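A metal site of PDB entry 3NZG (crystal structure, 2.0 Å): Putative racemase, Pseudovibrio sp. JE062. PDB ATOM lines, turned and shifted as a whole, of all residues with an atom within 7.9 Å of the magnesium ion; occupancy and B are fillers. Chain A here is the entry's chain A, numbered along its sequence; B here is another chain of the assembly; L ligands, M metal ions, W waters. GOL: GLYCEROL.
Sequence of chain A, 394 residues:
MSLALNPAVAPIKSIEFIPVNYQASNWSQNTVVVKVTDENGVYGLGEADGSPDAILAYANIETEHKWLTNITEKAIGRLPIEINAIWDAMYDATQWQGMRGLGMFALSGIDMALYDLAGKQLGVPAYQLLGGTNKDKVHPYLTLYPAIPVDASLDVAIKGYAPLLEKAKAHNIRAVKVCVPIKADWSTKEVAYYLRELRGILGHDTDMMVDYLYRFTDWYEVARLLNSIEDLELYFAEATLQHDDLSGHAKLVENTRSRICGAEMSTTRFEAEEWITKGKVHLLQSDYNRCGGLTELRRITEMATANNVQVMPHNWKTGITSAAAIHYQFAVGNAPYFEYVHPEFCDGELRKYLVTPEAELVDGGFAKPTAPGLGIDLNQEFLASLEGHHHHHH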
ATOM      1  N   TYR A 141     -15.752 -21.921   7.855  1.00  0.00           N
ATOM      2  CA  TYR A 141     -15.592 -23.347   8.047  1.00  0.00           C
ATOM      3  C   TYR A 141     -14.074 -23.405   7.968  1.00  0.00           C
ATOM      4  O   TYR A 141     -13.467 -22.630   7.231  1.00  0.00           O
ATOM      5  CB  TYR A 141     -16.284 -24.169   6.940  1.00  0.00           C
ATOM      6  CG  TYR A 141     -15.621 -24.257   5.586  1.00  0.00           C
ATOM      7  CD1 TYR A 141     -14.506 -25.083   5.378  1.00  0.00           C
ATOM      8  CD2 TYR A 141     -16.151 -23.588   4.477  1.00  0.00           C
ATOM      9  CE1 TYR A 141     -13.959 -25.256   4.100  1.00  0.00           C
ATOM     10  CE2 TYR A 141     -15.613 -23.757   3.201  1.00  0.00           C
ATOM     11  CZ  TYR A 141     -14.514 -24.593   3.024  1.00  0.00           C
ATOM     12  OH  TYR A 141     -13.981 -24.757   1.764  1.00  0.00           O
ATOM     13  N   THR A 143     -10.595 -25.425   7.157  1.00  0.00           N
ATOM     14  CA  THR A 143     -10.043 -26.556   6.449  1.00  0.00           C
ATOM     15  C   THR A 143      -8.940 -27.149   7.287  1.00  0.00           C
ATOM     16  O   THR A 143      -7.932 -26.496   7.554  1.00  0.00           O
ATOM     17  CB  THR A 143      -9.474 -26.140   5.077  1.00  0.00           C
ATOM     18  OG1 THR A 143     -10.511 -25.558   4.286  1.00  0.00           O
ATOM     19  CG2 THR A 143      -8.921 -27.351   4.355  1.00  0.00           C
ATOM     20  N   LYS A 177     -13.567 -28.726   7.240  1.00  0.00           N
ATOM     21  CA  LYS A 177     -13.391 -29.510   6.012  1.00  0.00           C
ATOM     22  C   LYS A 177     -12.218 -30.464   6.145  1.00  0.00           C
ATOM     23  O   LYS A 177     -11.125 -30.054   6.535  1.00  0.00           O
ATOM     24  CB  LYS A 177     -13.158 -28.586   4.809  1.00  0.00           C
ATOM     25  CG  LYS A 177     -13.038 -29.347   3.482  1.00  0.00           C
ATOM     26  CD  LYS A 177     -13.136 -28.442   2.259  1.00  0.00           C
ATOM     27  CE  LYS A 177     -11.841 -27.691   1.971  1.00  0.00           C
ATOM     28  NZ  LYS A 177     -12.018 -26.701   0.867  1.00  0.00           N
ATOM     29  N   CYS A 179      -9.890 -33.669   4.214  1.00  0.00           N
ATOM     30  CA  CYS A 179      -9.450 -34.068   2.874  1.00  0.00           C
ATOM     31  C   CYS A 179      -9.064 -35.537   2.808  1.00  0.00           C
ATOM     32  O   CYS A 179      -8.731 -36.147   3.817  1.00  0.00           O
ATOM     33  CB  CYS A 179      -8.233 -33.242   2.462  1.00  0.00           C
ATOM     34  SG  CYS A 179      -8.367 -31.459   2.680  1.00  0.00           S
ATOM     35  N   VAL A 210     -16.143 -32.177   2.724  1.00  0.00           N
ATOM     36  CA  VAL A 210     -15.089 -33.082   2.293  1.00  0.00           C
ATOM     37  C   VAL A 210     -14.487 -32.688   0.952  1.00  0.00           C
ATOM     38  O   VAL A 210     -15.207 -32.431  -0.022  1.00  0.00           O
ATOM     39  CB  VAL A 210     -15.598 -34.541   2.202  1.00  0.00           C
ATOM     40  CG1 VAL A 210     -14.477 -35.456   1.748  1.00  0.00           C
ATOM     41  CG2 VAL A 210     -16.129 -34.989   3.551  1.00  0.00           C
ATOM     42  N   ASP A 211     -13.159 -32.637   0.921  1.00  0.00           N
ATOM     43  CA  ASP A 211     -12.394 -32.311  -0.276  1.00  0.00           C
ATOM     44  C   ASP A 211     -11.764 -33.630  -0.729  1.00  0.00           C
ATOM     45  O   ASP A 211     -11.000 -34.242   0.030  1.00  0.00           O
ATOM     46  CB  ASP A 211     -11.291 -31.295   0.068  1.00  0.00           C
ATOM     47  CG  ASP A 211     -10.622 -30.711  -1.160  1.00  0.00           C
ATOM     48  OD1 ASP A 211     -10.334 -31.473  -2.111  1.00  0.00           O
ATOM     49  OD2 ASP A 211     -10.355 -29.490  -1.162  1.00  0.00           O
ATOM     50  N   TYR A 212     -12.083 -34.077  -1.941  1.00  0.00           N
ATOM     51  CA  TYR A 212     -11.545 -35.339  -2.434  1.00  0.00           C
ATOM     52  C   TYR A 212     -10.299 -35.153  -3.297  1.00  0.00           C
ATOM     53  O   TYR A 212      -9.762 -36.113  -3.848  1.00  0.00           O
ATOM     54  CB  TYR A 212     -12.625 -36.090  -3.229  1.00  0.00           C
ATOM     55  CG  TYR A 212     -13.822 -36.468  -2.384  1.00  0.00           C
ATOM     56  CD1 TYR A 212     -13.888 -37.711  -1.762  1.00  0.00           C
ATOM     57  CD2 TYR A 212     -14.880 -35.576  -2.210  1.00  0.00           C
ATOM     58  CE1 TYR A 212     -14.977 -38.055  -0.964  1.00  0.00           C
ATOM     59  CE2 TYR A 212     -15.965 -35.907  -1.416  1.00  0.00           C
ATOM     60  CZ  TYR A 212     -16.010 -37.143  -0.803  1.00  0.00           C
ATOM     61  OH  TYR A 212     -17.073 -37.472  -0.009  1.00  0.00           O
ATOM     62  N   LEU A 213      -9.845 -33.910  -3.395  1.00  0.00           N
ATOM     63  CA  LEU A 213      -8.640 -33.590  -4.147  1.00  0.00           C
ATOM     64  C   LEU A 213      -8.520 -34.196  -5.543  1.00  0.00           C
ATOM     65  O   LEU A 213      -7.439 -34.642  -5.936  1.00  0.00           O
ATOM     66  CB  LEU A 213      -7.414 -33.961  -3.298  1.00  0.00           C
ATOM     67  CG  LEU A 213      -7.322 -33.176  -1.986  1.00  0.00           C
ATOM     68  CD1 LEU A 213      -6.182 -33.716  -1.118  1.00  0.00           C
ATOM     69  CD2 LEU A 213      -7.126 -31.700  -2.296  1.00  0.00           C
ATOM     70  N   TYR A 214      -9.627 -34.223  -6.272  1.00  0.00           N
ATOM     71  CA  TYR A 214      -9.649 -34.712  -7.654  1.00  0.00           C
ATOM     72  C   TYR A 214      -9.126 -36.120  -7.882  1.00  0.00           C
ATOM     73  O   TYR A 214      -8.427 -36.372  -8.855  1.00  0.00           O
ATOM     74  CB  TYR A 214      -8.869 -33.728  -8.533  1.00  0.00           C
ATOM     75  CG  TYR A 214      -9.353 -32.302  -8.415  1.00  0.00           C
ATOM     76  CD1 TYR A 214     -10.595 -31.913  -8.932  1.00  0.00           C
ATOM     77  CD2 TYR A 214      -8.573 -31.329  -7.776  1.00  0.00           C
ATOM     78  CE1 TYR A 214     -11.052 -30.606  -8.808  1.00  0.00           C
ATOM     79  CE2 TYR A 214      -9.026 -30.019  -7.638  1.00  0.00           C
ATOM     80  CZ  TYR A 214     -10.270 -29.663  -8.163  1.00  0.00           C
ATOM     81  OH  TYR A 214     -10.742 -28.384  -8.020  1.00  0.00           O
ATOM     82  N   PHE A 236     -20.878 -30.896   1.921  1.00  0.00           N
ATOM     83  CA  PHE A 236     -20.636 -30.917   0.480  1.00  0.00           C
ATOM     84  C   PHE A 236     -19.516 -31.861   0.056  1.00  0.00           C
ATOM     85  O   PHE A 236     -18.766 -32.375   0.877  1.00  0.00           O
ATOM     86  CB  PHE A 236     -20.405 -29.489  -0.064  1.00  0.00           C
ATOM     87  CG  PHE A 236     -19.099 -28.819   0.366  1.00  0.00           C
ATOM     88  CD1 PHE A 236     -17.871 -29.481   0.275  1.00  0.00           C
ATOM     89  CD2 PHE A 236     -19.101 -27.483   0.730  1.00  0.00           C
ATOM     90  CE1 PHE A 236     -16.680 -28.807   0.539  1.00  0.00           C
ATOM     91  CE2 PHE A 236     -17.919 -26.806   0.997  1.00  0.00           C
ATOM     92  CZ  PHE A 236     -16.694 -27.476   0.901  1.00  0.00           C
ATOM     93  N   GLU A 238     -16.431 -31.721  -2.433  1.00  0.00           N
ATOM     94  CA  GLU A 238     -15.582 -30.868  -3.258  1.00  0.00           C
ATOM     95  C   GLU A 238     -14.523 -31.654  -4.029  1.00  0.00           C
ATOM     96  O   GLU A 238     -14.057 -32.705  -3.579  1.00  0.00           O
ATOM     97  CB  GLU A 238     -14.888 -29.811  -2.381  1.00  0.00           C
ATOM     98  CG  GLU A 238     -13.669 -29.121  -2.997  1.00  0.00           C
ATOM     99  CD  GLU A 238     -13.043 -28.095  -2.051  1.00  0.00           C
ATOM    100  OE1 GLU A 238     -13.590 -27.892  -0.955  1.00  0.00           O
ATOM    101  OE2 GLU A 238     -12.015 -27.484  -2.404  1.00  0.00           O
ATOM    102  N   ALA A 239     -14.182 -31.145  -5.205  1.00  0.00           N
ATOM    103  CA  ALA A 239     -13.171 -31.745  -6.056  1.00  0.00           C
ATOM    104  C   ALA A 239     -13.329 -33.259  -6.235  1.00  0.00           C
ATOM    105  O   ALA A 239     -12.375 -34.017  -6.068  1.00  0.00           O
ATOM    106  CB  ALA A 239     -11.777 -31.434  -5.504  1.00  0.00           C
ATOM    107  N   GLU A 264     -13.404 -24.362  -8.105  1.00  0.00           N
ATOM    108  CA  GLU A 264     -12.307 -24.033  -7.209  1.00  0.00           C
ATOM    109  C   GLU A 264     -11.122 -23.374  -7.936  1.00  0.00           C
ATOM    110  O   GLU A 264     -10.568 -22.387  -7.446  1.00  0.00           O
ATOM    111  CB  GLU A 264     -11.829 -25.311  -6.489  1.00  0.00           C
ATOM    112  CG  GLU A 264     -10.569 -25.114  -5.665  1.00  0.00           C
ATOM    113  CD  GLU A 264     -10.175 -26.369  -4.888  1.00  0.00           C
ATOM    114  OE1 GLU A 264     -10.182 -27.461  -5.489  1.00  0.00           O
ATOM    115  OE2 GLU A 264      -9.859 -26.249  -3.679  1.00  0.00           O
ATOM    116  N   MET A 265     -10.755 -23.910  -9.107  1.00  0.00           N
ATOM    117  CA  MET A 265      -9.616 -23.367  -9.856  1.00  0.00           C
ATOM    118  C   MET A 265      -9.989 -22.503 -11.069  1.00  0.00           C
ATOM    119  O   MET A 265      -9.124 -22.178 -11.896  1.00  0.00           O
ATOM    120  CB  MET A 265      -8.718 -24.515 -10.342  1.00  0.00           C
ATOM    121  CG  MET A 265      -8.270 -25.477  -9.244  1.00  0.00           C
ATOM    122  SD  MET A 265      -6.982 -26.805  -9.876  1.00  0.00           S
ATOM    123  CE  MET A 265      -8.190 -28.131 -10.618  1.00  0.00           C
ATOM    124  N   GLN A 285     -16.686 -22.284  -5.784  1.00  0.00           N
ATOM    125  CA  GLN A 285     -15.542 -22.009  -4.925  1.00  0.00           C
ATOM    126  C   GLN A 285     -14.484 -21.094  -5.564  1.00  0.00           C
ATOM    127  O   GLN A 285     -13.312 -21.163  -5.208  1.00  0.00           O
ATOM    128  CB  GLN A 285     -14.924 -23.331  -4.493  1.00  0.00           C
ATOM    129  CG  GLN A 285     -15.945 -24.236  -3.815  1.00  0.00           C
ATOM    130  CD  GLN A 285     -15.379 -25.543  -3.321  1.00  0.00           C
ATOM    131  OE1 GLN A 285     -14.854 -26.338  -4.100  1.00  0.00           O
ATOM    132  NE2 GLN A 285     -15.492 -25.781  -2.029  1.00  0.00           N
ATOM    133  N   HIS A 314     -12.776 -20.315  -2.485  1.00  0.00           N
ATOM    134  CA  HIS A 314     -11.594 -21.063  -2.082  1.00  0.00           C
ATOM    135  C   HIS A 314     -10.661 -20.065  -1.404  1.00  0.00           C
ATOM    136  O   HIS A 314     -10.568 -18.910  -1.835  1.00  0.00           O
ATOM    137  CB  HIS A 314     -10.916 -21.659  -3.317  1.00  0.00           C
ATOM    138  CG  HIS A 314      -9.566 -22.253  -3.044  1.00  0.00           C
ATOM    139  ND1 HIS A 314      -9.397 -23.483  -2.457  1.00  0.00           N
ATOM    140  CD2 HIS A 314      -8.313 -21.756  -3.251  1.00  0.00           C
ATOM    141  CE1 HIS A 314      -8.108 -23.733  -2.307  1.00  0.00           C
ATOM    142  NE2 HIS A 314      -7.433 -22.703  -2.782  1.00  0.00           N
ATOM    143  N   ASN A 315      -9.958 -20.494  -0.359  1.00  0.00           N
ATOM    144  CA  ASN A 315      -9.063 -19.593   0.344  1.00  0.00           C
ATOM    145  C   ASN A 315      -7.993 -20.324   1.122  1.00  0.00           C
ATOM    146  O   ASN A 315      -8.259 -20.940   2.154  1.00  0.00           O
ATOM    147  CB  ASN A 315      -9.890 -18.696   1.283  1.00  0.00           C
ATOM    148  CG  ASN A 315      -9.021 -17.861   2.231  1.00  0.00           C
ATOM    149  OD1 ASN A 315      -7.877 -17.525   1.920  1.00  0.00           O
ATOM    150  ND2 ASN A 315      -9.582 -17.493   3.384  1.00  0.00           N
ATOM    151  N   TRP A 316      -6.769 -20.275   0.601  1.00  0.00           N
ATOM    152  CA  TRP A 316      -5.624 -20.891   1.244  1.00  0.00           C
ATOM    153  C   TRP A 316      -4.361 -20.142   0.815  1.00  0.00           C
ATOM    154  O   TRP A 316      -3.577 -20.629  -0.005  1.00  0.00           O
ATOM    155  CB  TRP A 316      -5.495 -22.372   0.884  1.00  0.00           C
ATOM    156  CG  TRP A 316      -4.399 -23.032   1.669  1.00  0.00           C
ATOM    157  CD1 TRP A 316      -3.065 -23.021   1.375  1.00  0.00           C
ATOM    158  CD2 TRP A 316      -4.531 -23.709   2.924  1.00  0.00           C
ATOM    159  NE1 TRP A 316      -2.358 -23.636   2.386  1.00  0.00           N
ATOM    160  CE2 TRP A 316      -3.233 -24.071   3.346  1.00  0.00           C
ATOM    161  CE3 TRP A 316      -5.634 -24.038   3.732  1.00  0.00           C
ATOM    162  CZ2 TRP A 316      -2.999 -24.752   4.544  1.00  0.00           C
ATOM    163  CZ3 TRP A 316      -5.400 -24.719   4.930  1.00  0.00           C
ATOM    164  CH2 TRP A 316      -4.082 -25.065   5.326  1.00  0.00           C
ATOM    165  N   GLU A 339     -14.832 -20.446   3.355  1.00  0.00           N
ATOM    166  CA  GLU A 339     -13.522 -21.013   3.683  1.00  0.00           C
ATOM    167  C   GLU A 339     -12.575 -20.035   4.359  1.00  0.00           C
ATOM    168  O   GLU A 339     -12.499 -18.857   3.991  1.00  0.00           O
ATOM    169  CB  GLU A 339     -12.827 -21.592   2.446  1.00  0.00           C
ATOM    170  CG  GLU A 339     -11.430 -22.156   2.733  1.00  0.00           C
ATOM    171  CD  GLU A 339     -10.945 -23.156   1.687  1.00  0.00           C
ATOM    172  OE1 GLU A 339     -11.034 -22.867   0.468  1.00  0.00           O
ATOM    173  OE2 GLU A 339     -10.469 -24.242   2.103  1.00  0.00           O
ATOM    174  N   TRP B  67      -0.359 -30.275  -8.982  1.00  0.00           N
ATOM    175  CA  TRP B  67      -0.983 -29.442 -10.006  1.00  0.00           C
ATOM    176  C   TRP B  67      -0.208 -28.194 -10.400  1.00  0.00           C
ATOM    177  O   TRP B  67      -0.636 -27.455 -11.285  1.00  0.00           O
ATOM    178  CB  TRP B  67      -2.388 -29.049  -9.536  1.00  0.00           C
ATOM    179  CG  TRP B  67      -3.236 -30.243  -9.302  1.00  0.00           C
ATOM    180  CD1 TRP B  67      -3.656 -31.129 -10.237  1.00  0.00           C
ATOM    181  CD2 TRP B  67      -3.743 -30.701  -8.044  1.00  0.00           C
ATOM    182  NE1 TRP B  67      -4.387 -32.134  -9.647  1.00  0.00           N
ATOM    183  CE2 TRP B  67      -4.461 -31.889  -8.304  1.00  0.00           C
ATOM    184  CE3 TRP B  67      -3.668 -30.228  -6.725  1.00  0.00           C
ATOM    185  CZ2 TRP B  67      -5.101 -32.619  -7.288  1.00  0.00           C
ATOM    186  CZ3 TRP B  67      -4.300 -30.955  -5.720  1.00  0.00           C
ATOM    187  CH2 TRP B  67      -5.002 -32.134  -6.010  1.00  0.00           C
ATOM    188  N   TRP B  96      -3.130 -26.136 -11.954  1.00  0.00           N
ATOM    189  CA  TRP B  96      -3.267 -24.993 -11.049  1.00  0.00           C
ATOM    190  C   TRP B  96      -3.185 -23.640 -11.746  1.00  0.00           C
ATOM    191  O   TRP B  96      -3.821 -22.674 -11.312  1.00  0.00           O
ATOM    192  CB  TRP B  96      -2.223 -25.072  -9.931  1.00  0.00           C
ATOM    193  CG  TRP B  96      -2.559 -24.166  -8.791  1.00  0.00           C
ATOM    194  CD1 TRP B  96      -2.008 -22.943  -8.508  1.00  0.00           C
ATOM    195  CD2 TRP B  96      -3.565 -24.376  -7.798  1.00  0.00           C
ATOM    196  NE1 TRP B  96      -2.607 -22.384  -7.409  1.00  0.00           N
ATOM    197  CE2 TRP B  96      -3.578 -23.237  -6.952  1.00  0.00           C
ATOM    198  CE3 TRP B  96      -4.475 -25.424  -7.539  1.00  0.00           C
ATOM    199  CZ2 TRP B  96      -4.456 -23.120  -5.871  1.00  0.00           C
ATOM    200  CZ3 TRP B  96      -5.350 -25.294  -6.461  1.00  0.00           C
ATOM    201  CH2 TRP B  96      -5.329 -24.157  -5.644  1.00  0.00           C
HETATM  202  C1  GOL L   1      -7.320 -27.363  -1.335  1.00  0.00           C
HETATM  203  O1  GOL L   1      -7.934 -27.824  -2.520  1.00  0.00           O
HETATM  204  C2  GOL L   1      -8.340 -27.126  -0.202  1.00  0.00           C
HETATM  205  O2  GOL L   1      -9.585 -26.595  -0.677  1.00  0.00           O
HETATM  206  C3  GOL L   1      -7.725 -26.163   0.776  1.00  0.00           C
HETATM  207  O3  GOL L   1      -8.682 -25.183   1.080  1.00  0.00           O
HETATM  208 MG    MG M   1      -9.907 -27.892  -2.386  1.00  0.00          MG
HETATM  209  O   HOH W   1      -9.545 -29.309  -3.695  1.00  0.00           O
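OD1 of Asp 211 sits at hydrogen-bond distance from N of Leu 213, 2.8 Å away. The side-chain carboxylate (OE2) of Glu 264 sits close to a ring nitrogen (ND1) of His 314 (3.1 Å). The backbone carbonyl oxygen of Glu 238 lies within hydrogen-bond range of the backbone NH of Tyr 212, 2.9 Å away. N of Glu 238 lies within hydrogen-bond range of O of Val 210 (2.8 Å). The side-chain hydroxyl (OH) of Tyr 214 lies within hydrogen-bond range of the side-chain carboxylate (OE1) of Glu 264 (2.8 Å). The side-chain carboxylate (OE1) of Glu 238 sits at hydrogen-bond distance from the side-chain amide nitrogen (NE2) of Gln 285, 3.0 Å away. OD2 of Asp 211 lies close to NZ of Lys 177 (3.8 Å). The side-chain carboxylate (OE1) of Glu 238 is in salt-bridge range of the side-chain amino group (NZ) of Lys 177, at 2.7 Å.
Of the 21 residues printed, 3 come within 4 Å of the magnesium ion.
The magnesium ion is bound by water W1 (2.0 Å), O1 of the ligand (2.0 Å), OD2 of Asp 211 (2.1 Å), OE2 of Glu 264 (2.1 Å), OE2 of Glu 238 (2.1 Å) and O2 of the ligand (2.2 Å).
Water W1 lies within hydrogen-bond range of the side-chain carboxylate (OE1) of Glu 264 (2.7 Å) and the side-chain carboxylate (OD1) of Asp 211 (2.8 Å).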
